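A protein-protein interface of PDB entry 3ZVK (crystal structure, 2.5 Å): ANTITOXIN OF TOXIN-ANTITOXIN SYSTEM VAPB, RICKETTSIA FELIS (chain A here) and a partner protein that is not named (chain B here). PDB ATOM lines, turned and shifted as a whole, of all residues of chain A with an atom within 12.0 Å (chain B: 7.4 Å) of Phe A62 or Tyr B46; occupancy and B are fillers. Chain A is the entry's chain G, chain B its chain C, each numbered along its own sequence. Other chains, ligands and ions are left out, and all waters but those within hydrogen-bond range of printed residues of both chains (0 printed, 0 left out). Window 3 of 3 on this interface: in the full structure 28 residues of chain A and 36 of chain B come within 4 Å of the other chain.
Printed residues of chain B within 4 Å of Phe A62: Val B11, Glu B43, Tyr B46, Gly B47 and Lys B50. Printed residues of chain A within 4 Å of Tyr B46: Phe A62 (3.6 Å). Val B11 touches just one residue of chain A: Phe A62. No residue of chain A comes within 4 Å of Ala B42. Of the printed residues of chain A, Glu B43 touches Phe A62 (3.2 Å) and Arg A66 (2.8 Å). Leu B44 touches none of the printed residues of chain A. Gln B45 touches one residue of chain A. Of chain A, only Ile A61 (3.6 Å) and Phe A62 (3.9 Å) come within 4 Å of Gly B47. No residue of chain A comes within 4 Å of Val B48. No residue of chain A comes within 4 Å of Ser B49. Lys B50 touches one residue of chain A. Of the printed residues of chain B, Leu A33 touches Gln B45. Printed residues of chain B within 4 Å of Ile A61: Asn B15 (3.0 Å), Gly B47 (3.6 Å) and Asn B57 (3.7 Å).
Of the 18 printed residues of chain B, 11 touch a printed residue of chain A. Hydrophobic or aromatic side chains of chain B within 4 Å of the printed part of chain A: Val B11 and Tyr B46. Printed residues of chain A that touch a printed residue of chain B: Leu A33, Ser A58, Asp A59, Asp A60, Ile A61, Phe A62, Arg A66 and Asp A68. Hydrophobic or aromatic side chains of chain A that line the printed part of chain B: Leu A33, Ile A61 and Phe A62. Along chain A the printed residues that touch a printed residue of chain B span positions 33 to 68. Among the printed residues, Asp or Glu carboxylates within 4 Å of a Lys or Arg side-chain nitrogen of the other chain: Arg A66 with Glu B43 (2.8 Å).
The side-chain amide nitrogen (ND2) of Asn B15 lies within hydrogen-bond range of the backbone carbonyl oxygen (O) of Ile A61. NH2 of Arg A66 is in salt-bridge range of OE2 of Glu B43. OD1 of Asn B57 sits at hydrogen-bond distance from OG of Ser A58, 2.7 Å away. The side-chain amide oxygen (OD1) of Asn B57 sits close to the backbone carbonyl oxygen (O) of Asp A59 (3.2 Å). The side-chain carboxylate (OD1) of Asp A68 lies within hydrogen-bond range of the backbone NH (N) of Asn B98, at 2.8 Å.
Among the printed residues, pairs that only touch across the chains: Phe A62 with Glu B43 (3.2 Å), Asp A60 with Asn B15 (3.4 Å), Arg A66 with Thr B7 (3.5 Å), Ile A61 with Gly B47 (3.6 Å), Phe A62 with Tyr B46 (3.6 Å), Phe A62 with Lys B50 (3.6 Å), Leu A33 with Gln B45 (3.7 Å), Ile A61 with Asn B57 (3.7 Å), Phe A62 with Val B11 (3.7 Å), Asp A59 with Ser B51 (3.7 Å) and Phe A62 with Gly B47 (3.9 Å).
The side-chain hydroxyl (OG1) of Thr B7 lies within hydrogen-bond range of the side-chain carboxylate (OE2) of Glu B43 (2.7 Å). The side-chain carboxylate (OE1) of Glu B43 sits at hydrogen-bond distance from the side-chain amide nitrogen (ND2) of Asn B98 (3.2 Å). The backbone carbonyl oxygen of Gln B45 is in hydrogen-bond range of the side-chain hydroxyl of Ser B49 (3.3 Å). O of Val B48 sits at hydrogen-bond distance from OG of Ser B51, 2.7 Å away. The side-chain amide nitrogen (ND2) of Asn B57 is in hydrogen-bond range of the side-chain hydroxyl (OG) of Ser B51 (2.9 Å). NH2 of Arg A66 is in salt-bridge range of OD2 of Asp A68.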
ATOM      1  N   PRO A  32      20.484 -11.238  20.850  1.00  0.00           N
ATOM      2  CA  PRO A  32      19.998 -10.423  19.725  1.00  0.00           C
ATOM      3  C   PRO A  32      19.995 -11.210  18.411  1.00  0.00           C
ATOM      4  O   PRO A  32      20.799 -12.126  18.231  1.00  0.00           O
ATOM      5  CB  PRO A  32      20.983  -9.251  19.687  1.00  0.00           C
ATOM      6  CG  PRO A  32      22.243  -9.794  20.282  1.00  0.00           C
ATOM      7  CD  PRO A  32      21.872 -10.879  21.235  1.00  0.00           C
ATOM      8  N   LEU A  33      19.068 -10.874  17.506  1.00  0.00           N
ATOM      9  CA  LEU A  33      18.945 -11.493  16.186  1.00  0.00           C
ATOM     10  C   LEU A  33      18.279 -10.451  15.301  1.00  0.00           C
ATOM     11  O   LEU A  33      17.076 -10.201  15.424  1.00  0.00           O
ATOM     12  CB  LEU A  33      18.148 -12.817  16.249  1.00  0.00           C
ATOM     13  CG  LEU A  33      18.064 -13.658  14.984  1.00  0.00           C
ATOM     14  CD1 LEU A  33      19.406 -14.265  14.645  1.00  0.00           C
ATOM     15  CD2 LEU A  33      17.073 -14.790  15.183  1.00  0.00           C
ATOM     16  N   GLY A  34      19.091  -9.785  14.484  1.00  0.00           N
ATOM     17  CA  GLY A  34      18.630  -8.696  13.629  1.00  0.00           C
ATOM     18  C   GLY A  34      18.067  -7.566  14.468  1.00  0.00           C
ATOM     19  O   GLY A  34      18.667  -7.212  15.479  1.00  0.00           O
ATOM     20  N   SER A  58      21.804 -31.384  12.879  1.00  0.00           N
ATOM     21  CA  SER A  58      21.870 -30.475  11.736  1.00  0.00           C
ATOM     22  C   SER A  58      23.115 -30.736  10.906  1.00  0.00           C
ATOM     23  O   SER A  58      24.031 -31.422  11.370  1.00  0.00           O
ATOM     24  CB  SER A  58      21.864 -29.016  12.199  1.00  0.00           C
ATOM     25  OG  SER A  58      23.012 -28.670  12.960  1.00  0.00           O
ATOM     26  N   ASP A  59      23.164 -30.140   9.697  1.00  0.00           N
ATOM     27  CA  ASP A  59      24.352 -30.191   8.853  1.00  0.00           C
ATOM     28  C   ASP A  59      25.409 -29.242   9.445  1.00  0.00           C
ATOM     29  O   ASP A  59      25.061 -28.302  10.166  1.00  0.00           O
ATOM     30  CB  ASP A  59      24.033 -29.894   7.364  1.00  0.00           C
ATOM     31  CG  ASP A  59      23.595 -28.489   6.970  1.00  0.00           C
ATOM     32  OD1 ASP A  59      22.700 -27.925   7.647  1.00  0.00           O
ATOM     33  OD2 ASP A  59      24.089 -27.987   5.936  1.00  0.00           O
ATOM     34  N   ASP A  60      26.693 -29.535   9.209  1.00  0.00           N
ATOM     35  CA  ASP A  60      27.795 -28.722   9.721  1.00  0.00           C
ATOM     36  C   ASP A  60      27.862 -27.379   9.021  1.00  0.00           C
ATOM     37  O   ASP A  60      27.652 -27.306   7.807  1.00  0.00           O
ATOM     38  CB  ASP A  60      29.139 -29.463   9.552  1.00  0.00           C
ATOM     39  CG  ASP A  60      29.444 -30.563  10.572  1.00  0.00           C
ATOM     40  OD1 ASP A  60      28.650 -30.733  11.537  1.00  0.00           O
ATOM     41  OD2 ASP A  60      30.502 -31.216  10.439  1.00  0.00           O
ATOM     42  N   ILE A  61      28.144 -26.326   9.785  1.00  0.00           N
ATOM     43  CA  ILE A  61      28.336 -24.968   9.259  1.00  0.00           C
ATOM     44  C   ILE A  61      29.772 -24.945   8.715  1.00  0.00           C
ATOM     45  O   ILE A  61      30.638 -25.638   9.271  1.00  0.00           O
ATOM     46  CB  ILE A  61      28.032 -23.858  10.319  1.00  0.00           C
ATOM     47  CG1 ILE A  61      28.862 -24.035  11.616  1.00  0.00           C
ATOM     48  CG2 ILE A  61      26.516 -23.768  10.605  1.00  0.00           C
ATOM     49  CD1 ILE A  61      28.987 -22.744  12.517  1.00  0.00           C
ATOM     50  N   PHE A  62      30.007 -24.240   7.586  1.00  0.00           N
ATOM     51  CA  PHE A  62      31.311 -24.179   6.902  1.00  0.00           C
ATOM     52  C   PHE A  62      31.875 -25.600   6.555  1.00  0.00           C
ATOM     53  O   PHE A  62      32.972 -25.939   7.028  1.00  0.00           O
ATOM     54  CB  PHE A  62      32.327 -23.365   7.738  1.00  0.00           C
ATOM     55  CG  PHE A  62      32.004 -21.909   7.941  1.00  0.00           C
ATOM     56  CD1 PHE A  62      32.180 -20.989   6.913  1.00  0.00           C
ATOM     57  CD2 PHE A  62      31.595 -21.442   9.182  1.00  0.00           C
ATOM     58  CE1 PHE A  62      31.907 -19.636   7.110  1.00  0.00           C
ATOM     59  CE2 PHE A  62      31.343 -20.080   9.389  1.00  0.00           C
ATOM     60  CZ  PHE A  62      31.504 -19.186   8.353  1.00  0.00           C
ATOM     61  N   PRO A  63      31.150 -26.459   5.779  1.00  0.00           N
ATOM     62  CA  PRO A  63      31.661 -27.824   5.512  1.00  0.00           C
ATOM     63  C   PRO A  63      32.943 -27.859   4.700  1.00  0.00           C
ATOM     64  O   PRO A  63      33.751 -28.778   4.860  1.00  0.00           O
ATOM     65  CB  PRO A  63      30.515 -28.505   4.753  1.00  0.00           C
ATOM     66  CG  PRO A  63      29.329 -27.652   4.944  1.00  0.00           C
ATOM     67  CD  PRO A  63      29.838 -26.256   5.125  1.00  0.00           C
ATOM     68  N   GLU A  64      33.107 -26.867   3.818  1.00  0.00           N
ATOM     69  CA  GLU A  64      34.263 -26.689   2.953  1.00  0.00           C
ATOM     70  C   GLU A  64      35.303 -25.812   3.662  1.00  0.00           C
ATOM     71  O   GLU A  64      36.454 -25.740   3.218  1.00  0.00           O
ATOM     72  CB  GLU A  64      33.836 -26.059   1.615  1.00  0.00           C
ATOM     73  N   GLY A  65      34.888 -25.174   4.758  1.00  0.00           N
ATOM     74  CA  GLY A  65      35.742 -24.300   5.555  1.00  0.00           C
ATOM     75  C   GLY A  65      35.421 -22.829   5.415  1.00  0.00           C
ATOM     76  O   GLY A  65      34.455 -22.452   4.744  1.00  0.00           O
ATOM     77  N   ARG A  66      36.225 -21.985   6.068  1.00  0.00           N
ATOM     78  CA  ARG A  66      36.058 -20.532   6.038  1.00  0.00           C
ATOM     79  C   ARG A  66      36.791 -19.927   4.854  1.00  0.00           C
ATOM     80  O   ARG A  66      37.959 -20.256   4.626  1.00  0.00           O
ATOM     81  CB  ARG A  66      36.593 -19.926   7.323  1.00  0.00           C
ATOM     82  CG  ARG A  66      35.574 -19.831   8.435  1.00  0.00           C
ATOM     83  CD  ARG A  66      36.246 -19.289   9.671  1.00  0.00           C
ATOM     84  NE  ARG A  66      36.609 -17.871   9.538  1.00  0.00           N
ATOM     85  CZ  ARG A  66      37.729 -17.336  10.013  1.00  0.00           C
ATOM     86  NH1 ARG A  66      38.613 -18.088  10.649  1.00  0.00           N
ATOM     87  NH2 ARG A  66      37.959 -16.036   9.881  1.00  0.00           N
ATOM     88  N   LYS A  67      36.111 -19.040   4.106  1.00  0.00           N
ATOM     89  CA  LYS A  67      36.682 -18.356   2.938  1.00  0.00           C
ATOM     90  C   LYS A  67      37.087 -16.948   3.368  1.00  0.00           C
ATOM     91  O   LYS A  67      36.441 -15.972   2.971  1.00  0.00           O
ATOM     92  CB  LYS A  67      35.670 -18.289   1.777  1.00  0.00           C
ATOM     93  CG  LYS A  67      35.316 -19.628   1.127  1.00  0.00           C
ATOM     94  CD  LYS A  67      34.583 -19.460  -0.225  1.00  0.00           C
ATOM     95  CE  LYS A  67      33.093 -19.161  -0.122  1.00  0.00           C
ATOM     96  NZ  LYS A  67      32.430 -19.176  -1.454  1.00  0.00           N
ATOM     97  N   ASP A  68      38.123 -16.831   4.223  1.00  0.00           N
ATOM     98  CA  ASP A  68      38.538 -15.509   4.699  1.00  0.00           C
ATOM     99  C   ASP A  68      39.675 -14.990   3.812  1.00  0.00           C
ATOM    100  O   ASP A  68      40.843 -15.289   4.063  1.00  0.00           O
ATOM    101  CB  ASP A  68      38.863 -15.519   6.219  1.00  0.00           C
ATOM    102  CG  ASP A  68      38.983 -14.149   6.856  1.00  0.00           C
ATOM    103  OD1 ASP A  68      38.459 -13.164   6.271  1.00  0.00           O
ATOM    104  OD2 ASP A  68      39.577 -14.057   7.946  1.00  0.00           O
ATOM    105  N   LEU A  69      39.308 -14.307   2.708  1.00  0.00           N
ATOM    106  CA  LEU A  69      40.273 -13.778   1.740  1.00  0.00           C
ATOM    107  C   LEU A  69      40.955 -12.530   2.311  1.00  0.00           C
ATOM    108  O   LEU A  69      40.362 -11.880   3.170  1.00  0.00           O
ATOM    109  CB  LEU A  69      39.574 -13.441   0.403  1.00  0.00           C
ATOM    110  CG  LEU A  69      39.141 -14.603  -0.500  1.00  0.00           C
ATOM    111  CD1 LEU A  69      38.523 -14.076  -1.787  1.00  0.00           C
ATOM    112  CD2 LEU A  69      40.322 -15.555  -0.845  1.00  0.00           C
ATOM    113  N   THR B   7      36.955 -17.551  15.468  1.00  0.00           N
ATOM    114  CA  THR B   7      35.942 -18.225  14.652  1.00  0.00           C
ATOM    115  C   THR B   7      36.105 -19.727  14.620  1.00  0.00           C
ATOM    116  O   THR B   7      35.125 -20.436  14.819  1.00  0.00           O
ATOM    117  CB  THR B   7      35.806 -17.588  13.245  1.00  0.00           C
ATOM    118  OG1 THR B   7      35.672 -16.167  13.375  1.00  0.00           O
ATOM    119  CG2 THR B   7      34.580 -18.114  12.474  1.00  0.00           C
ATOM    120  N   VAL B  11      33.277 -22.500  15.533  1.00  0.00           N
ATOM    121  CA  VAL B  11      32.797 -23.440  14.523  1.00  0.00           C
ATOM    122  C   VAL B  11      32.980 -24.890  15.022  1.00  0.00           C
ATOM    123  O   VAL B  11      32.026 -25.666  14.952  1.00  0.00           O
ATOM    124  CB  VAL B  11      33.483 -23.189  13.153  1.00  0.00           C
ATOM    125  CG1 VAL B  11      33.200 -24.322  12.150  1.00  0.00           C
ATOM    126  CG2 VAL B  11      33.073 -21.842  12.573  1.00  0.00           C
ATOM    127  N   ASN B  15      29.881 -27.416  15.805  1.00  0.00           N
ATOM    128  CA  ASN B  15      29.840 -28.645  15.024  1.00  0.00           C
ATOM    129  C   ASN B  15      30.200 -29.901  15.788  1.00  0.00           C
ATOM    130  O   ASN B  15      29.448 -30.866  15.720  1.00  0.00           O
ATOM    131  CB  ASN B  15      30.690 -28.530  13.763  1.00  0.00           C
ATOM    132  CG  ASN B  15      30.152 -27.589  12.713  1.00  0.00           C
ATOM    133  OD1 ASN B  15      28.962 -27.299  12.628  1.00  0.00           O
ATOM    134  ND2 ASN B  15      31.025 -27.130  11.848  1.00  0.00           N
ATOM    135  N   VAL B  40      33.228 -12.209  14.812  1.00  0.00           N
ATOM    136  CA  VAL B  40      33.087 -13.662  14.913  1.00  0.00           C
ATOM    137  C   VAL B  40      31.621 -13.994  14.685  1.00  0.00           C
ATOM    138  O   VAL B  40      31.327 -14.863  13.872  1.00  0.00           O
ATOM    139  CB  VAL B  40      33.611 -14.236  16.267  1.00  0.00           C
ATOM    140  CG1 VAL B  40      33.205 -15.703  16.455  1.00  0.00           C
ATOM    141  CG2 VAL B  40      35.129 -14.075  16.381  1.00  0.00           C
ATOM    142  N   LEU B  41      30.706 -13.256  15.354  1.00  0.00           N
ATOM    143  CA  LEU B  41      29.262 -13.464  15.240  1.00  0.00           C
ATOM    144  C   LEU B  41      28.765 -13.267  13.819  1.00  0.00           C
ATOM    145  O   LEU B  41      27.917 -14.040  13.369  1.00  0.00           O
ATOM    146  CB  LEU B  41      28.480 -12.626  16.271  1.00  0.00           C
ATOM    147  CG  LEU B  41      26.958 -12.829  16.293  1.00  0.00           C
ATOM    148  CD1 LEU B  41      26.564 -14.297  16.588  1.00  0.00           C
ATOM    149  CD2 LEU B  41      26.295 -11.815  17.188  1.00  0.00           C
ATOM    150  N   ALA B  42      29.352 -12.288  13.086  1.00  0.00           N
ATOM    151  CA  ALA B  42      29.042 -12.028  11.672  1.00  0.00           C
ATOM    152  C   ALA B  42      29.349 -13.267  10.863  1.00  0.00           C
ATOM    153  O   ALA B  42      28.512 -13.687  10.064  1.00  0.00           O
ATOM    154  CB  ALA B  42      29.849 -10.848  11.159  1.00  0.00           C
ATOM    155  N   GLU B  43      30.512 -13.904  11.128  1.00  0.00           N
ATOM    156  CA  GLU B  43      30.944 -15.137  10.460  1.00  0.00           C
ATOM    157  C   GLU B  43      30.037 -16.312  10.792  1.00  0.00           C
ATOM    158  O   GLU B  43      29.660 -17.048   9.876  1.00  0.00           O
ATOM    159  CB  GLU B  43      32.396 -15.485  10.813  1.00  0.00           C
ATOM    160  CG  GLU B  43      33.383 -14.492  10.251  1.00  0.00           C
ATOM    161  CD  GLU B  43      34.725 -15.103   9.970  1.00  0.00           C
ATOM    162  OE1 GLU B  43      34.915 -15.616   8.843  1.00  0.00           O
ATOM    163  OE2 GLU B  43      35.580 -15.080  10.886  1.00  0.00           O
ATOM    164  N   LEU B  44      29.680 -16.485  12.089  1.00  0.00           N
ATOM    165  CA  LEU B  44      28.815 -17.579  12.541  1.00  0.00           C
ATOM    166  C   LEU B  44      27.392 -17.436  12.025  1.00  0.00           C
ATOM    167  O   LEU B  44      26.774 -18.447  11.697  1.00  0.00           O
ATOM    168  CB  LEU B  44      28.823 -17.737  14.063  1.00  0.00           C
ATOM    169  CG  LEU B  44      30.151 -17.991  14.737  1.00  0.00           C
ATOM    170  CD1 LEU B  44      29.979 -17.991  16.256  1.00  0.00           C
ATOM    171  CD2 LEU B  44      30.796 -19.280  14.245  1.00  0.00           C
ATOM    172  N   GLN B  45      26.883 -16.184  11.911  1.00  0.00           N
ATOM    173  CA  GLN B  45      25.567 -15.913  11.318  1.00  0.00           C
ATOM    174  C   GLN B  45      25.578 -16.241   9.817  1.00  0.00           C
ATOM    175  O   GLN B  45      24.594 -16.776   9.313  1.00  0.00           O
ATOM    176  CB  GLN B  45      25.096 -14.469  11.567  1.00  0.00           C
ATOM    177  CG  GLN B  45      24.455 -14.240  12.932  1.00  0.00           C
ATOM    178  CD  GLN B  45      23.200 -15.044  13.199  1.00  0.00           C
ATOM    179  OE1 GLN B  45      22.902 -15.400  14.338  1.00  0.00           O
ATOM    180  NE2 GLN B  45      22.447 -15.380  12.165  1.00  0.00           N
ATOM    181  N   TYR B  46      26.704 -15.984   9.128  1.00  0.00           N
ATOM    182  CA  TYR B  46      26.858 -16.339   7.714  1.00  0.00           C
ATOM    183  C   TYR B  46      26.879 -17.855   7.540  1.00  0.00           C
ATOM    184  O   TYR B  46      26.271 -18.351   6.597  1.00  0.00           O
ATOM    185  CB  TYR B  46      28.078 -15.646   7.090  1.00  0.00           C
ATOM    186  CG  TYR B  46      28.621 -16.305   5.840  1.00  0.00           C
ATOM    187  CD1 TYR B  46      27.897 -16.294   4.642  1.00  0.00           C
ATOM    188  CD2 TYR B  46      29.872 -16.912   5.839  1.00  0.00           C
ATOM    189  CE1 TYR B  46      28.392 -16.911   3.491  1.00  0.00           C
ATOM    190  CE2 TYR B  46      30.387 -17.507   4.687  1.00  0.00           C
ATOM    191  CZ  TYR B  46      29.656 -17.478   3.508  1.00  0.00           C
ATOM    192  OH  TYR B  46      30.150 -18.088   2.376  1.00  0.00           O
ATOM    193  N   GLY B  47      27.518 -18.567   8.471  1.00  0.00           N
ATOM    194  CA  GLY B  47      27.563 -20.029   8.501  1.00  0.00           C
ATOM    195  C   GLY B  47      26.171 -20.638   8.605  1.00  0.00           C
ATOM    196  O   GLY B  47      25.848 -21.582   7.878  1.00  0.00           O
ATOM    197  N   VAL B  48      25.313 -20.036   9.450  1.00  0.00           N
ATOM    198  CA  VAL B  48      23.904 -20.425   9.652  1.00  0.00           C
ATOM    199  C   VAL B  48      23.086 -20.193   8.365  1.00  0.00           C
ATOM    200  O   VAL B  48      22.422 -21.112   7.895  1.00  0.00           O
ATOM    201  CB  VAL B  48      23.278 -19.685  10.890  1.00  0.00           C
ATOM    202  CG1 VAL B  48      21.758 -19.852  10.952  1.00  0.00           C
ATOM    203  CG2 VAL B  48      23.929 -20.134  12.197  1.00  0.00           C
ATOM    204  N   SER B  49      23.126 -18.967   7.817  1.00  0.00           N
ATOM    205  CA  SER B  49      22.370 -18.569   6.616  1.00  0.00           C
ATOM    206  C   SER B  49      22.702 -19.398   5.364  1.00  0.00           C
ATOM    207  O   SER B  49      21.829 -19.642   4.525  1.00  0.00           O
ATOM    208  CB  SER B  49      22.568 -17.082   6.331  1.00  0.00           C
ATOM    209  OG  SER B  49      22.001 -16.290   7.361  1.00  0.00           O
ATOM    210  N   LYS B  50      23.968 -19.816   5.254  1.00  0.00           N
ATOM    211  CA  LYS B  50      24.514 -20.603   4.149  1.00  0.00           C
ATOM    212  C   LYS B  50      24.072 -22.080   4.216  1.00  0.00           C
ATOM    213  O   LYS B  50      23.914 -22.704   3.178  1.00  0.00           O
ATOM    214  CB  LYS B  50      26.045 -20.477   4.191  1.00  0.00           C
ATOM    215  CG  LYS B  50      26.767 -21.100   3.034  1.00  0.00           C
ATOM    216  CD  LYS B  50      28.186 -20.600   2.953  1.00  0.00           C
ATOM    217  CE  LYS B  50      29.215 -21.475   3.640  1.00  0.00           C
ATOM    218  NZ  LYS B  50      29.079 -21.464   5.120  1.00  0.00           N
ATOM    219  N   SER B  51      23.916 -22.638   5.426  1.00  0.00           N
ATOM    220  CA  SER B  51      23.553 -24.040   5.670  1.00  0.00           C
ATOM    221  C   SER B  51      22.159 -24.469   5.162  1.00  0.00           C
ATOM    222  O   SER B  51      21.346 -23.619   4.785  1.00  0.00           O
ATOM    223  CB  SER B  51      23.710 -24.364   7.151  1.00  0.00           C
ATOM    224  OG  SER B  51      22.662 -23.799   7.921  1.00  0.00           O
ATOM    225  N   ASN B  57      20.682 -24.837  13.094  1.00  0.00           N
ATOM    226  CA  ASN B  57      21.973 -24.191  13.238  1.00  0.00           C
ATOM    227  C   ASN B  57      21.860 -22.878  13.994  1.00  0.00           C
ATOM    228  O   ASN B  57      22.712 -22.582  14.825  1.00  0.00           O
ATOM    229  CB  ASN B  57      22.699 -24.081  11.898  1.00  0.00           C
ATOM    230  CG  ASN B  57      23.290 -25.401  11.427  1.00  0.00           C
ATOM    231  OD1 ASN B  57      23.813 -26.197  12.224  1.00  0.00           O
ATOM    232  ND2 ASN B  57      23.264 -25.657  10.115  1.00  0.00           N
ATOM    233  N   LEU B  61      23.654 -22.089  17.589  1.00  0.00           N
ATOM    234  CA  LEU B  61      24.384 -20.838  17.764  1.00  0.00           C
ATOM    235  C   LEU B  61      23.811 -20.044  18.967  1.00  0.00           C
ATOM    236  O   LEU B  61      24.595 -19.580  19.797  1.00  0.00           O
ATOM    237  CB  LEU B  61      24.351 -20.008  16.460  1.00  0.00           C
ATOM    238  CG  LEU B  61      24.980 -18.597  16.480  1.00  0.00           C
ATOM    239  CD1 LEU B  61      26.422 -18.627  16.930  1.00  0.00           C
ATOM    240  CD2 LEU B  61      24.893 -17.951  15.139  1.00  0.00           C
ATOM    241  N   ASN B  98      38.730 -11.075   8.062  1.00  0.00           N
ATOM    242  CA  ASN B  98      38.020 -11.199   9.322  1.00  0.00           C
ATOM    243  C   ASN B  98      38.954 -11.483  10.472  1.00  0.00           C
ATOM    244  O   ASN B  98      38.845 -10.818  11.490  1.00  0.00           O
ATOM    245  CB  ASN B  98      36.871 -12.201   9.215  1.00  0.00           C
ATOM    246  CG  ASN B  98      35.706 -11.699   8.393  1.00  0.00           C
ATOM    247  OD1 ASN B  98      35.466 -10.500   8.253  1.00  0.00           O
ATOM    248  ND2 ASN B  98      34.942 -12.599   7.827  1.00  0.00           N
